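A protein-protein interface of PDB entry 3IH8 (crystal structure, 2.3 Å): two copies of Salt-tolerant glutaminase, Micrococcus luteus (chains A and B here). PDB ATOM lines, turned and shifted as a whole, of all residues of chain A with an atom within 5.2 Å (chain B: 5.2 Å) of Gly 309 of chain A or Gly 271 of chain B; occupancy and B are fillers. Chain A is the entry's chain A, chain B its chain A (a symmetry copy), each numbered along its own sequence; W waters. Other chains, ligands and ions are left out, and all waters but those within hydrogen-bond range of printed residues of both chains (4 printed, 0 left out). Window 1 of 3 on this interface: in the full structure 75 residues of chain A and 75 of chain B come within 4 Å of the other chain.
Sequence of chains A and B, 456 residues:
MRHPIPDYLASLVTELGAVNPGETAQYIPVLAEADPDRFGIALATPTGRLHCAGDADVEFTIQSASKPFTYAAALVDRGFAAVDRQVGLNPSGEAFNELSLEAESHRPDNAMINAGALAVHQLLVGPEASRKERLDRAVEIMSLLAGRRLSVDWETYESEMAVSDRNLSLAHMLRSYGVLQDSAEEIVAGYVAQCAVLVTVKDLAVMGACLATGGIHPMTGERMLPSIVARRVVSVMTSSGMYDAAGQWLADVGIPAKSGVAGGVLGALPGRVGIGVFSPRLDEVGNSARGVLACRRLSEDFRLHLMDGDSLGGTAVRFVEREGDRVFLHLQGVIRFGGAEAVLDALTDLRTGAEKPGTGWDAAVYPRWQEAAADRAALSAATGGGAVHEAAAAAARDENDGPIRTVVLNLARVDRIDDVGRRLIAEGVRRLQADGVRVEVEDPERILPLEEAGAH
No position is printed for both chains.
Of the 7 pairs that touch across the chains among the printed residues, none has its exchanged pair printed and touching as well.
Hydrophobic or aromatic side chains of chain B that line the printed part of chain A: Pro 270.
Along chain B the printed residues that touch a printed residue of chain A span positions 270 to 336.
Among the printed residues, 7 pairs touch across the chains.
Among the printed residues, Asp or Glu carboxylates within 4 Å of a Lys or Arg side-chain nitrogen of the other chain: Asp 308 of chain A with Arg 336 of chain B.
Of the printed residues of chain B, Met 307 of chain A touches Pro 270.
Gly 309 of chain A touches just one residue of chain B: Gly 271 (3.6 Å).
Pro 46 of chain B touches none of the printed residues of chain A.
Of the printed residues of chain A, Arg 272 of chain B touches Ser 311.
The nearest residue of chain B that does not touch Gly 309 of chain A is Pro 270 of chain B (4.1 Å).
The nearest printed residue of chain B that does not touch Asp 310 of chain A is Val 334 of chain B (4.9 Å).
Water W2 lies within hydrogen-bond range of OG of Ser 311 of chain A and NE of Arg 272 of chain B.
Water W4 lies within hydrogen-bond range of the side-chain carboxylate (OD2) of Asp 310 of chain A (2.8 Å), the backbone carbonyl oxygen (O) of Val 334 of chain B (3.1 Å) and the backbone NH (N) of Arg 336 of chain B (3.2 Å).
Water W3 bridges the backbone carbonyl oxygen of Ser 311 of chain A (2.9 Å) and the backbone NH of Val 334 of chain B (3.2 Å).
Water W1 bridges OD2 of Asp 310 of chain A (3.0 Å) and O of Val 334 of chain B (3.3 Å).
The backbone carbonyl oxygen (O) of Ala 212 of chain B is in hydrogen-bond range of the backbone NH (N) of Gly 271 of chain B, at 2.7 Å.
NH1 of Arg 336 of chain B lies within salt-bridge range of OD2 of Asp 308 of chain A, 3.0 Å away.
The side-chain hydroxyl (OG) of Ser 311 of chain A sits close to the backbone carbonyl oxygen (O) of Gly 271 of chain B (3.5 Å).
Met 307 of chain A touches Pro 270 of chain B.
O of Asp 308 of chain A touches CB of Pro 270 of chain B, at 3.7 Å.
Gly 271 of chain B touches Gly 309 of chain A (N to CA, 3.6 Å).
Asp 310 of chain A touches Arg 336 of chain B (OD2 to CB, 3.8 Å).
Ser 311 of chain A touches Arg 272 of chain B.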
ATOM      1  N   MET A 307     -19.778 -27.822   3.661  1.00  0.00           N
ATOM      2  CA  MET A 307     -20.318 -26.964   4.709  1.00  0.00           C
ATOM      3  C   MET A 307     -21.841 -26.987   4.835  1.00  0.00           C
ATOM      4  O   MET A 307     -22.412 -26.164   5.540  1.00  0.00           O
ATOM      5  CB  MET A 307     -19.854 -25.521   4.507  1.00  0.00           C
ATOM      6  CG  MET A 307     -18.342 -25.330   4.525  1.00  0.00           C
ATOM      7  SD  MET A 307     -17.543 -26.117   5.952  1.00  0.00           S
ATOM      8  CE  MET A 307     -15.931 -26.419   5.309  1.00  0.00           C
ATOM      9  N   ASP A 308     -22.498 -27.925   4.158  1.00  0.00           N
ATOM     10  CA  ASP A 308     -23.955 -28.038   4.221  1.00  0.00           C
ATOM     11  C   ASP A 308     -24.438 -28.514   5.586  1.00  0.00           C
ATOM     12  O   ASP A 308     -23.815 -29.372   6.216  1.00  0.00           O
ATOM     13  CB  ASP A 308     -24.448 -29.034   3.183  1.00  0.00           C
ATOM     14  CG  ASP A 308     -24.231 -28.560   1.771  1.00  0.00           C
ATOM     15  OD1 ASP A 308     -24.139 -29.426   0.864  1.00  0.00           O
ATOM     16  OD2 ASP A 308     -24.170 -27.326   1.570  1.00  0.00           O
ATOM     17  N   GLY A 309     -25.560 -27.967   6.037  1.00  0.00           N
ATOM     18  CA  GLY A 309     -26.103 -28.378   7.320  1.00  0.00           C
ATOM     19  C   GLY A 309     -27.034 -29.569   7.155  1.00  0.00           C
ATOM     20  O   GLY A 309     -28.062 -29.656   7.822  1.00  0.00           O
ATOM     21  N   ASP A 310     -26.664 -30.494   6.272  1.00  0.00           N
ATOM     22  CA  ASP A 310     -27.470 -31.683   5.999  1.00  0.00           C
ATOM     23  C   ASP A 310     -27.334 -32.752   7.098  1.00  0.00           C
ATOM     24  O   ASP A 310     -26.678 -33.778   6.904  1.00  0.00           O
ATOM     25  CB  ASP A 310     -27.058 -32.263   4.641  1.00  0.00           C
ATOM     26  CG  ASP A 310     -28.085 -33.222   4.083  1.00  0.00           C
ATOM     27  OD1 ASP A 310     -28.506 -34.139   4.818  1.00  0.00           O
ATOM     28  OD2 ASP A 310     -28.470 -33.064   2.907  1.00  0.00           O
ATOM     29  N   SER A 311     -27.973 -32.515   8.241  1.00  0.00           N
ATOM     30  CA  SER A 311     -27.890 -33.441   9.372  1.00  0.00           C
ATOM     31  C   SER A 311     -29.248 -33.921   9.862  1.00  0.00           C
ATOM     32  O   SER A 311     -30.248 -33.229   9.713  1.00  0.00           O
ATOM     33  CB  SER A 311     -27.162 -32.771  10.543  1.00  0.00           C
ATOM     34  OG  SER A 311     -25.871 -32.317  10.161  1.00  0.00           O
ATOM     35  N   PRO B  46     -28.863 -26.200  16.836  1.00  0.00           N
ATOM     36  CA  PRO B  46     -29.666 -25.633  15.741  1.00  0.00           C
ATOM     37  C   PRO B  46     -31.091 -25.305  16.193  1.00  0.00           C
ATOM     38  O   PRO B  46     -31.628 -24.231  15.895  1.00  0.00           O
ATOM     39  CB  PRO B  46     -29.665 -26.745  14.695  1.00  0.00           C
ATOM     40  CG  PRO B  46     -28.388 -27.489  14.976  1.00  0.00           C
ATOM     41  CD  PRO B  46     -28.362 -27.539  16.473  1.00  0.00           C
ATOM     42  N   ALA B 212     -23.535 -22.405  11.662  1.00  0.00           N
ATOM     43  CA  ALA B 212     -23.683 -23.858  11.550  1.00  0.00           C
ATOM     44  C   ALA B 212     -24.975 -24.272  10.858  1.00  0.00           C
ATOM     45  O   ALA B 212     -25.043 -25.337  10.240  1.00  0.00           O
ATOM     46  CB  ALA B 212     -23.624 -24.500  12.932  1.00  0.00           C
ATOM     47  N   THR B 213     -25.998 -23.436  10.966  1.00  0.00           N
ATOM     48  CA  THR B 213     -27.297 -23.745  10.369  1.00  0.00           C
ATOM     49  C   THR B 213     -27.453 -23.246   8.944  1.00  0.00           C
ATOM     50  O   THR B 213     -28.490 -23.472   8.322  1.00  0.00           O
ATOM     51  CB  THR B 213     -28.445 -23.124  11.190  1.00  0.00           C
ATOM     52  OG1 THR B 213     -28.333 -21.692  11.153  1.00  0.00           O
ATOM     53  CG2 THR B 213     -28.382 -23.601  12.632  1.00  0.00           C
ATOM     54  N   LEU B 269     -19.823 -25.836  13.563  1.00  0.00           N
ATOM     55  CA  LEU B 269     -19.849 -27.114  12.847  1.00  0.00           C
ATOM     56  C   LEU B 269     -21.185 -27.221  12.124  1.00  0.00           C
ATOM     57  O   LEU B 269     -22.225 -27.392  12.749  1.00  0.00           O
ATOM     58  CB  LEU B 269     -19.698 -28.274  13.837  1.00  0.00           C
ATOM     59  CG  LEU B 269     -19.689 -29.702  13.277  1.00  0.00           C
ATOM     60  CD1 LEU B 269     -18.446 -29.951  12.426  1.00  0.00           C
ATOM     61  CD2 LEU B 269     -19.712 -30.672  14.441  1.00  0.00           C
ATOM     62  N   PRO B 270     -21.174 -27.121  10.789  1.00  0.00           N
ATOM     63  CA  PRO B 270     -22.414 -27.205  10.017  1.00  0.00           C
ATOM     64  C   PRO B 270     -23.348 -28.338  10.420  1.00  0.00           C
ATOM     65  O   PRO B 270     -22.933 -29.495  10.574  1.00  0.00           O
ATOM     66  CB  PRO B 270     -21.913 -27.339   8.587  1.00  0.00           C
ATOM     67  CG  PRO B 270     -20.685 -26.487   8.610  1.00  0.00           C
ATOM     68  CD  PRO B 270     -20.019 -26.946   9.890  1.00  0.00           C
ATOM     69  N   GLY B 271     -24.616 -27.980  10.596  1.00  0.00           N
ATOM     70  CA  GLY B 271     -25.633 -28.950  10.959  1.00  0.00           C
ATOM     71  C   GLY B 271     -25.646 -29.452  12.388  1.00  0.00           C
ATOM     72  O   GLY B 271     -26.592 -30.132  12.767  1.00  0.00           O
ATOM     73  N   ARG B 272     -24.632 -29.137  13.195  1.00  0.00           N
ATOM     74  CA  ARG B 272     -24.633 -29.632  14.568  1.00  0.00           C
ATOM     75  C   ARG B 272     -24.596 -28.648  15.713  1.00  0.00           C
ATOM     76  O   ARG B 272     -25.513 -28.628  16.532  1.00  0.00           O
ATOM     77  CB  ARG B 272     -23.501 -30.632  14.800  1.00  0.00           C
ATOM     78  CG  ARG B 272     -23.681 -31.959  14.099  1.00  0.00           C
ATOM     79  CD  ARG B 272     -23.253 -31.857  12.647  1.00  0.00           C
ATOM     80  NE  ARG B 272     -22.667 -33.112  12.201  1.00  0.00           N
ATOM     81  CZ  ARG B 272     -21.601 -33.681  12.750  1.00  0.00           C
ATOM     82  NH1 ARG B 272     -20.977 -33.119  13.769  1.00  0.00           N
ATOM     83  NH2 ARG B 272     -21.175 -34.841  12.298  1.00  0.00           N
ATOM     84  N   VAL B 273     -23.555 -27.824  15.789  1.00  0.00           N
ATOM     85  CA  VAL B 273     -23.468 -26.927  16.932  1.00  0.00           C
ATOM     86  C   VAL B 273     -22.664 -25.647  16.780  1.00  0.00           C
ATOM     87  O   VAL B 273     -21.810 -25.518  15.905  1.00  0.00           O
ATOM     88  CB  VAL B 273     -22.909 -27.711  18.157  1.00  0.00           C
ATOM     89  CG1 VAL B 273     -21.474 -28.153  17.881  1.00  0.00           C
ATOM     90  CG2 VAL B 273     -22.972 -26.864  19.407  1.00  0.00           C
ATOM     91  N   VAL B 334     -34.987 -32.069   6.800  1.00  0.00           N
ATOM     92  CA  VAL B 334     -34.462 -30.964   6.007  1.00  0.00           C
ATOM     93  C   VAL B 334     -34.006 -31.557   4.680  1.00  0.00           C
ATOM     94  O   VAL B 334     -32.961 -32.207   4.608  1.00  0.00           O
ATOM     95  CB  VAL B 334     -33.275 -30.287   6.725  1.00  0.00           C
ATOM     96  CG1 VAL B 334     -32.597 -29.276   5.796  1.00  0.00           C
ATOM     97  CG2 VAL B 334     -33.771 -29.604   7.995  1.00  0.00           C
ATOM     98  N   ARG B 336     -32.503 -31.571   1.041  1.00  0.00           N
ATOM     99  CA  ARG B 336     -31.588 -30.934   0.111  1.00  0.00           C
ATOM    100  C   ARG B 336     -31.244 -32.066  -0.845  1.00  0.00           C
ATOM    101  O   ARG B 336     -32.000 -33.033  -0.950  1.00  0.00           O
ATOM    102  CB  ARG B 336     -30.333 -30.431   0.827  1.00  0.00           C
ATOM    103  CG  ARG B 336     -30.627 -29.434   1.935  1.00  0.00           C
ATOM    104  CD  ARG B 336     -29.404 -28.586   2.271  1.00  0.00           C
ATOM    105  NE  ARG B 336     -29.101 -27.637   1.200  1.00  0.00           N
ATOM    106  CZ  ARG B 336     -28.005 -26.889   1.142  1.00  0.00           C
ATOM    107  NH1 ARG B 336     -27.093 -26.973   2.099  1.00  0.00           N
ATOM    108  NH2 ARG B 336     -27.818 -26.057   0.125  1.00  0.00           N
HETATM  109  O   HOH W   1     -29.866 -31.148   4.687  1.00  0.00           O
HETATM  110  O   HOH W   2     -23.706 -33.901   9.594  1.00  0.00           O
HETATM  111  O   HOH W   3     -33.015 -33.386   9.018  1.00  0.00           O
HETATM  112  O   HOH W   4     -31.115 -33.936   2.770  1.00  0.00           O
